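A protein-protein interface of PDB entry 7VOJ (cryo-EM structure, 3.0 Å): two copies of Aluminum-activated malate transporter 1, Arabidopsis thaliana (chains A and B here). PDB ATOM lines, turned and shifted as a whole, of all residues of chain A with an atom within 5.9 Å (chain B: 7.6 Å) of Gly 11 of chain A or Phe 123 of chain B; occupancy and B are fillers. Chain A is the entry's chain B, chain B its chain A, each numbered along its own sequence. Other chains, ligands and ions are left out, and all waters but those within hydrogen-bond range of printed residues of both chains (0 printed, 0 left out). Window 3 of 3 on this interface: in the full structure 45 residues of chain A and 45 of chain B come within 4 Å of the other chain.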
ATOM      1  N   GLU A   6      10.579   6.941 -12.255  1.00  0.00           N
ATOM      2  CA  GLU A   6      11.579   7.571 -11.398  1.00  0.00           C
ATOM      3  C   GLU A   6      10.989   7.990 -10.055  1.00  0.00           C
ATOM      4  O   GLU A   6      11.631   7.816  -9.011  1.00  0.00           O
ATOM      5  CB  GLU A   6      12.199   8.768 -12.109  1.00  0.00           C
ATOM      6  CG  GLU A   6      12.897   8.411 -13.410  1.00  0.00           C
ATOM      7  CD  GLU A   6      14.291   7.837 -13.203  1.00  0.00           C
ATOM      8  OE1 GLU A   6      14.830   7.952 -12.081  1.00  0.00           O
ATOM      9  OE2 GLU A   6      14.849   7.276 -14.171  1.00  0.00           O
ATOM     10  N   ILE A   7       9.754   8.496 -10.050  1.00  0.00           N
ATOM     11  CA  ILE A   7       9.187   8.935  -8.781  1.00  0.00           C
ATOM     12  C   ILE A   7       8.700   7.749  -7.944  1.00  0.00           C
ATOM     13  O   ILE A   7       8.745   7.810  -6.709  1.00  0.00           O
ATOM     14  CB  ILE A   7       8.086   9.988  -9.009  1.00  0.00           C
ATOM     15  CG1 ILE A   7       7.723  10.678  -7.693  1.00  0.00           C
ATOM     16  CG2 ILE A   7       6.858   9.394  -9.648  1.00  0.00           C
ATOM     17  CD1 ILE A   7       6.640  11.716  -7.814  1.00  0.00           C
ATOM     18  N   VAL A   8       8.309   6.628  -8.561  1.00  0.00           N
ATOM     19  CA  VAL A   8       7.916   5.511  -7.707  1.00  0.00           C
ATOM     20  C   VAL A   8       9.136   4.805  -7.127  1.00  0.00           C
ATOM     21  O   VAL A   8       9.075   4.291  -6.007  1.00  0.00           O
ATOM     22  CB  VAL A   8       6.983   4.517  -8.421  1.00  0.00           C
ATOM     23  CG1 VAL A   8       5.686   5.193  -8.813  1.00  0.00           C
ATOM     24  CG2 VAL A   8       7.642   3.866  -9.614  1.00  0.00           C
ATOM     25  N   ARG A   9      10.279   4.805  -7.822  1.00  0.00           N
ATOM     26  CA  ARG A   9      11.441   4.207  -7.176  1.00  0.00           C
ATOM     27  C   ARG A   9      12.064   5.150  -6.159  1.00  0.00           C
ATOM     28  O   ARG A   9      12.681   4.685  -5.190  1.00  0.00           O
ATOM     29  CB  ARG A   9      12.471   3.750  -8.208  1.00  0.00           C
ATOM     30  CG  ARG A   9      13.081   4.827  -9.055  1.00  0.00           C
ATOM     31  CD  ARG A   9      13.532   4.209 -10.360  1.00  0.00           C
ATOM     32  NE  ARG A   9      12.482   3.350 -10.898  1.00  0.00           N
ATOM     33  CZ  ARG A   9      12.604   2.610 -11.992  1.00  0.00           C
ATOM     34  NH1 ARG A   9      11.591   1.860 -12.401  1.00  0.00           N
ATOM     35  NH2 ARG A   9      13.738   2.619 -12.677  1.00  0.00           N
ATOM     36  N   GLU A  10      11.881   6.462  -6.331  1.00  0.00           N
ATOM     37  CA  GLU A  10      12.285   7.396  -5.287  1.00  0.00           C
ATOM     38  C   GLU A  10      11.436   7.222  -4.038  1.00  0.00           C
ATOM     39  O   GLU A  10      11.953   7.268  -2.914  1.00  0.00           O
ATOM     40  CB  GLU A  10      12.200   8.827  -5.805  1.00  0.00           C
ATOM     41  CG  GLU A  10      12.418   9.893  -4.757  1.00  0.00           C
ATOM     42  CD  GLU A  10      13.812   9.891  -4.186  1.00  0.00           C
ATOM     43  OE1 GLU A  10      14.758   9.494  -4.893  1.00  0.00           O
ATOM     44  OE2 GLU A  10      13.967  10.303  -3.024  1.00  0.00           O
ATOM     45  N   GLY A  11      10.137   6.983  -4.213  1.00  0.00           N
ATOM     46  CA  GLY A  11       9.295   6.667  -3.073  1.00  0.00           C
ATOM     47  C   GLY A  11       9.660   5.345  -2.434  1.00  0.00           C
ATOM     48  O   GLY A  11       9.565   5.192  -1.213  1.00  0.00           O
ATOM     49  N   ILE A  12      10.115   4.388  -3.246  1.00  0.00           N
ATOM     50  CA  ILE A  12      10.541   3.091  -2.731  1.00  0.00           C
ATOM     51  C   ILE A  12      11.766   3.242  -1.842  1.00  0.00           C
ATOM     52  O   ILE A  12      11.820   2.675  -0.745  1.00  0.00           O
ATOM     53  CB  ILE A  12      10.780   2.120  -3.901  1.00  0.00           C
ATOM     54  CG1 ILE A  12       9.476   1.434  -4.290  1.00  0.00           C
ATOM     55  CG2 ILE A  12      11.806   1.060  -3.566  1.00  0.00           C
ATOM     56  CD1 ILE A  12       9.606   0.558  -5.502  1.00  0.00           C
ATOM     57  N   ARG A  13      12.744   4.048  -2.262  1.00  0.00           N
ATOM     58  CA  ARG A  13      13.937   4.173  -1.432  1.00  0.00           C
ATOM     59  C   ARG A  13      13.702   5.073  -0.224  1.00  0.00           C
ATOM     60  O   ARG A  13      14.334   4.867   0.817  1.00  0.00           O
ATOM     61  CB  ARG A  13      15.135   4.657  -2.251  1.00  0.00           C
ATOM     62  CG  ARG A  13      15.151   6.109  -2.622  1.00  0.00           C
ATOM     63  CD  ARG A  13      16.554   6.650  -2.525  1.00  0.00           C
ATOM     64  NE  ARG A  13      16.919   6.880  -1.138  1.00  0.00           N
ATOM     65  CZ  ARG A  13      16.777   8.048  -0.525  1.00  0.00           C
ATOM     66  NH1 ARG A  13      17.127   8.180   0.744  1.00  0.00           N
ATOM     67  NH2 ARG A  13      16.292   9.087  -1.184  1.00  0.00           N
ATOM     68  N   VAL A  14      12.776   6.032  -0.316  1.00  0.00           N
ATOM     69  CA  VAL A  14      12.474   6.875   0.839  1.00  0.00           C
ATOM     70  C   VAL A  14      11.735   6.070   1.902  1.00  0.00           C
ATOM     71  O   VAL A  14      11.996   6.209   3.103  1.00  0.00           O
ATOM     72  CB  VAL A  14      11.692   8.123   0.386  1.00  0.00           C
ATOM     73  CG1 VAL A  14      10.984   8.798   1.534  1.00  0.00           C
ATOM     74  CG2 VAL A  14      12.634   9.106  -0.238  1.00  0.00           C
ATOM     75  N   GLY A  15      10.848   5.173   1.478  1.00  0.00           N
ATOM     76  CA  GLY A  15      10.199   4.299   2.436  1.00  0.00           C
ATOM     77  C   GLY A  15      11.136   3.252   3.003  1.00  0.00           C
ATOM     78  O   GLY A  15      11.082   2.945   4.195  1.00  0.00           O
ATOM     79  N   ASN A  16      12.015   2.696   2.162  1.00  0.00           N
ATOM     80  CA  ASN A  16      12.945   1.663   2.607  1.00  0.00           C
ATOM     81  C   ASN A  16      13.995   2.185   3.567  1.00  0.00           C
ATOM     82  O   ASN A  16      14.485   1.416   4.398  1.00  0.00           O
ATOM     83  CB  ASN A  16      13.654   1.030   1.412  1.00  0.00           C
ATOM     84  CG  ASN A  16      12.919  -0.170   0.869  1.00  0.00           C
ATOM     85  OD1 ASN A  16      12.542  -1.072   1.615  1.00  0.00           O
ATOM     86  ND2 ASN A  16      12.715  -0.194  -0.443  1.00  0.00           N
ATOM     87  N   ARG A  21       8.448   6.357   8.603  1.00  0.00           N
ATOM     88  CA  ARG A  21       7.817   7.390   7.800  1.00  0.00           C
ATOM     89  C   ARG A  21       6.459   6.937   7.292  1.00  0.00           C
ATOM     90  O   ARG A  21       5.523   7.738   7.207  1.00  0.00           O
ATOM     91  CB  ARG A  21       8.729   7.763   6.646  1.00  0.00           C
ATOM     92  CG  ARG A  21      10.060   8.239   7.129  1.00  0.00           C
ATOM     93  CD  ARG A  21      11.011   8.442   6.000  1.00  0.00           C
ATOM     94  NE  ARG A  21      12.272   8.976   6.478  1.00  0.00           N
ATOM     95  CZ  ARG A  21      13.322   9.184   5.700  1.00  0.00           C
ATOM     96  NH1 ARG A  21      13.255   8.894   4.412  1.00  0.00           N
ATOM     97  NH2 ARG A  21      14.435   9.677   6.212  1.00  0.00           N
ATOM     98  N   ILE A  22       6.321   5.649   6.981  1.00  0.00           N
ATOM     99  CA  ILE A  22       5.024   5.124   6.578  1.00  0.00           C
ATOM    100  C   ILE A  22       4.067   5.104   7.756  1.00  0.00           C
ATOM    101  O   ILE A  22       2.885   5.450   7.620  1.00  0.00           O
ATOM    102  CB  ILE A  22       5.179   3.725   5.972  1.00  0.00           C
ATOM    103  CG1 ILE A  22       6.317   3.706   4.972  1.00  0.00           C
ATOM    104  CG2 ILE A  22       3.916   3.331   5.279  1.00  0.00           C
ATOM    105  CD1 ILE A  22       6.549   2.351   4.376  1.00  0.00           C
ATOM    106  N   ALA A  25       2.907   8.646   8.407  1.00  0.00           N
ATOM    107  CA  ALA A  25       1.889   9.027   7.442  1.00  0.00           C
ATOM    108  C   ALA A  25       0.524   8.441   7.767  1.00  0.00           C
ATOM    109  O   ALA A  25      -0.485   9.081   7.483  1.00  0.00           O
ATOM    110  CB  ALA A  25       2.310   8.598   6.046  1.00  0.00           C
ATOM    111  N   GLN B 117      -5.547  11.586   1.219  1.00  0.00           N
ATOM    112  CA  GLN B 117      -4.698  12.698   0.807  1.00  0.00           C
ATOM    113  C   GLN B 117      -3.673  13.084   1.866  1.00  0.00           C
ATOM    114  O   GLN B 117      -2.515  13.344   1.553  1.00  0.00           O
ATOM    115  CB  GLN B 117      -5.519  13.926   0.424  1.00  0.00           C
ATOM    116  CG  GLN B 117      -4.695  14.967  -0.315  1.00  0.00           C
ATOM    117  CD  GLN B 117      -5.005  16.386   0.116  1.00  0.00           C
ATOM    118  OE1 GLN B 117      -5.844  16.614   0.986  1.00  0.00           O
ATOM    119  NE2 GLN B 117      -4.320  17.349  -0.488  1.00  0.00           N
ATOM    120  N   ALA B 118      -4.099  13.111   3.123  1.00  0.00           N
ATOM    121  CA  ALA B 118      -3.198  13.478   4.204  1.00  0.00           C
ATOM    122  C   ALA B 118      -2.061  12.477   4.299  1.00  0.00           C
ATOM    123  O   ALA B 118      -0.906  12.854   4.481  1.00  0.00           O
ATOM    124  CB  ALA B 118      -3.953  13.555   5.520  1.00  0.00           C
ATOM    125  N   ALA B 119      -2.392  11.197   4.180  1.00  0.00           N
ATOM    126  CA  ALA B 119      -1.383  10.154   4.230  1.00  0.00           C
ATOM    127  C   ALA B 119      -0.432  10.283   3.047  1.00  0.00           C
ATOM    128  O   ALA B 119       0.778  10.137   3.191  1.00  0.00           O
ATOM    129  CB  ALA B 119      -2.039   8.783   4.237  1.00  0.00           C
ATOM    130  N   LEU B 120      -0.994  10.559   1.875  1.00  0.00           N
ATOM    131  CA  LEU B 120      -0.196  10.702   0.661  1.00  0.00           C
ATOM    132  C   LEU B 120       0.770  11.888   0.687  1.00  0.00           C
ATOM    133  O   LEU B 120       1.898  11.785   0.216  1.00  0.00           O
ATOM    134  CB  LEU B 120      -1.103  10.783  -0.566  1.00  0.00           C
ATOM    135  CG  LEU B 120      -0.415  10.545  -1.909  1.00  0.00           C
ATOM    136  CD1 LEU B 120       0.197   9.155  -1.942  1.00  0.00           C
ATOM    137  CD2 LEU B 120      -1.401  10.725  -3.054  1.00  0.00           C
ATOM    138  N   SER B 121       0.313  13.010   1.234  1.00  0.00           N
ATOM    139  CA  SER B 121       1.097  14.234   1.305  1.00  0.00           C
ATOM    140  C   SER B 121       2.058  14.246   2.487  1.00  0.00           C
ATOM    141  O   SER B 121       3.159  14.797   2.372  1.00  0.00           O
ATOM    142  CB  SER B 121       0.170  15.432   1.357  1.00  0.00           C
ATOM    143  OG  SER B 121      -0.550  15.538   0.152  1.00  0.00           O
ATOM    144  N   THR B 122       1.691  13.633   3.614  1.00  0.00           N
ATOM    145  CA  THR B 122       2.630  13.545   4.723  1.00  0.00           C
ATOM    146  C   THR B 122       3.789  12.619   4.403  1.00  0.00           C
ATOM    147  O   THR B 122       4.895  12.819   4.909  1.00  0.00           O
ATOM    148  CB  THR B 122       1.921  13.068   5.973  1.00  0.00           C
ATOM    149  OG1 THR B 122       0.631  13.670   6.026  1.00  0.00           O
ATOM    150  CG2 THR B 122       2.677  13.482   7.182  1.00  0.00           C
ATOM    151  N   PHE B 123       3.571  11.613   3.558  1.00  0.00           N
ATOM    152  CA  PHE B 123       4.697  10.805   3.112  1.00  0.00           C
ATOM    153  C   PHE B 123       5.592  11.555   2.142  1.00  0.00           C
ATOM    154  O   PHE B 123       6.811  11.404   2.203  1.00  0.00           O
ATOM    155  CB  PHE B 123       4.208   9.517   2.464  1.00  0.00           C
ATOM    156  CG  PHE B 123       5.308   8.603   2.057  1.00  0.00           C
ATOM    157  CD1 PHE B 123       6.112   8.018   3.008  1.00  0.00           C
ATOM    158  CD2 PHE B 123       5.541   8.324   0.729  1.00  0.00           C
ATOM    159  CE1 PHE B 123       7.122   7.181   2.645  1.00  0.00           C
ATOM    160  CE2 PHE B 123       6.555   7.486   0.364  1.00  0.00           C
ATOM    161  CZ  PHE B 123       7.344   6.914   1.326  1.00  0.00           C
ATOM    162  N   VAL B 124       5.017  12.369   1.255  1.00  0.00           N
ATOM    163  CA  VAL B 124       5.820  13.126   0.299  1.00  0.00           C
ATOM    164  C   VAL B 124       6.633  14.227   0.985  1.00  0.00           C
ATOM    165  O   VAL B 124       7.699  14.608   0.494  1.00  0.00           O
ATOM    166  CB  VAL B 124       4.871  13.614  -0.815  1.00  0.00           C
ATOM    167  CG1 VAL B 124       5.461  14.674  -1.696  1.00  0.00           C
ATOM    168  CG2 VAL B 124       4.497  12.447  -1.680  1.00  0.00           C
ATOM    169  N   ARG B 125       6.237  14.665   2.177  1.00  0.00           N
ATOM    170  CA  ARG B 125       7.048  15.649   2.899  1.00  0.00           C
ATOM    171  C   ARG B 125       8.375  15.113   3.438  1.00  0.00           C
ATOM    172  O   ARG B 125       9.087  15.874   4.096  1.00  0.00           O
ATOM    173  CB  ARG B 125       6.261  16.227   4.066  1.00  0.00           C
ATOM    174  CG  ARG B 125       5.212  17.208   3.667  1.00  0.00           C
ATOM    175  CD  ARG B 125       4.492  17.725   4.866  1.00  0.00           C
ATOM    176  NE  ARG B 125       5.327  18.643   5.610  1.00  0.00           N
ATOM    177  CZ  ARG B 125       5.017  19.114   6.806  1.00  0.00           C
ATOM    178  NH1 ARG B 125       3.892  18.742   7.389  1.00  0.00           N
ATOM    179  NH2 ARG B 125       5.834  19.950   7.422  1.00  0.00           N
ATOM    180  N   PHE B 126       8.727  13.850   3.214  1.00  0.00           N
ATOM    181  CA  PHE B 126      10.023  13.315   3.597  1.00  0.00           C
ATOM    182  C   PHE B 126      10.990  13.220   2.431  1.00  0.00           C
ATOM    183  O   PHE B 126      12.148  12.860   2.643  1.00  0.00           O
ATOM    184  CB  PHE B 126       9.863  11.933   4.219  1.00  0.00           C
ATOM    185  CG  PHE B 126       9.157  11.936   5.530  1.00  0.00           C
ATOM    186  CD1 PHE B 126       9.820  12.296   6.679  1.00  0.00           C
ATOM    187  CD2 PHE B 126       7.840  11.553   5.615  1.00  0.00           C
ATOM    188  CE1 PHE B 126       9.178  12.288   7.880  1.00  0.00           C
ATOM    189  CE2 PHE B 126       7.198  11.545   6.816  1.00  0.00           C
ATOM    190  CZ  PHE B 126       7.869  11.914   7.946  1.00  0.00           C
ATOM    191  N   PHE B 127      10.533  13.500   1.215  1.00  0.00           N
ATOM    192  CA  PHE B 127      11.403  13.521   0.052  1.00  0.00           C
ATOM    193  C   PHE B 127      12.407  14.657   0.213  1.00  0.00           C
ATOM    194  O   PHE B 127      12.063  15.710   0.742  1.00  0.00           O
ATOM    195  CB  PHE B 127      10.609  13.763  -1.228  1.00  0.00           C
ATOM    196  CG  PHE B 127       9.881  12.568  -1.775  1.00  0.00           C
ATOM    197  CD1 PHE B 127       9.392  11.564  -0.966  1.00  0.00           C
ATOM    198  CD2 PHE B 127       9.663  12.480  -3.130  1.00  0.00           C
ATOM    199  CE1 PHE B 127       8.715  10.503  -1.496  1.00  0.00           C
ATOM    200  CE2 PHE B 127       8.987  11.416  -3.662  1.00  0.00           C
ATOM    201  CZ  PHE B 127       8.513  10.430  -2.840  1.00  0.00           C
ATOM    202  N   ILE B 138       3.267  21.745   0.701  1.00  0.00           N
ATOM    203  CA  ILE B 138       2.565  20.495   0.953  1.00  0.00           C
ATOM    204  C   ILE B 138       1.750  20.596   2.232  1.00  0.00           C
ATOM    205  O   ILE B 138       0.670  20.002   2.334  1.00  0.00           O
ATOM    206  CB  ILE B 138       3.553  19.318   0.988  1.00  0.00           C
ATOM    207  CG1 ILE B 138       4.449  19.346  -0.239  1.00  0.00           C
ATOM    208  CG2 ILE B 138       2.826  18.014   0.968  1.00  0.00           C
ATOM    209  CD1 ILE B 138       3.723  19.200  -1.544  1.00  0.00           C
ATOM    210  N   ILE B 142      -2.423  20.005   2.362  1.00  0.00           N
ATOM    211  CA  ILE B 142      -3.202  19.222   3.326  1.00  0.00           C
ATOM    212  C   ILE B 142      -4.267  20.082   3.985  1.00  0.00           C
ATOM    213  O   ILE B 142      -5.425  19.670   4.124  1.00  0.00           O
ATOM    214  CB  ILE B 142      -2.286  18.608   4.397  1.00  0.00           C
ATOM    215  CG1 ILE B 142      -1.192  17.766   3.791  1.00  0.00           C
ATOM    216  CG2 ILE B 142      -3.070  17.740   5.326  1.00  0.00           C
ATOM    217  CD1 ILE B 142      -0.171  17.356   4.804  1.00  0.00           C
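No position is printed for both chains.
Of the 6 pairs that touch across the chains among the printed residues, none has its exchanged pair printed and touching as well.
Of the 14 printed residues of chain A, 5 touch a printed residue of chain B.
Hydrophobic or aromatic side chains of chain B that line the printed part of chain A: Ala 119, Phe 123, Phe 126 and Phe 127.
Among the printed residues, no Asp or Glu carboxylate lies within 4 Å of a Lys or Arg side-chain nitrogen of the other chain.
Glu 10 of chain A touches Phe 127 of chain B (CG to CE2, 3.9 Å).
Gly 11 of chain A touches Phe 123 of chain B.
Gly 11 of chain A touches Phe 127 of chain B (CA to CZ, 3.9 Å).
N of Gly 15 of chain A touches CZ of Phe 123 of chain B, at 3.9 Å.
Arg 21 of chain A touches Phe 126 of chain B (CD to CG, 3.98 Å).
Ala 119 of chain B touches Ala 25 of chain A (CA to O, 3.5 Å).
Of chain B, only Phe 123 and Phe 127 come within 4 Å of Gly 11 of chain A.
Of the printed residues of chain B, Gly 15 of chain A touches Phe 123.
Of the printed residues of chain A, Phe 126 of chain B touches Arg 21 (3.98 Å).
Of the printed residues of chain A, Ala 119 of chain B touches Ala 25 (3.5 Å).
The nearest printed residue of chain B that does not touch Gly 11 of chain A is Val 124 of chain B (7.6 Å).
OE2 of Glu 10 of chain A lies within salt-bridge range of NH2 of Arg 13 of chain A (3.2 Å).
O of Val 14 of chain A sits at hydrogen-bond distance from NH1 of Arg 21 of chain A, at 3.2 Å.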
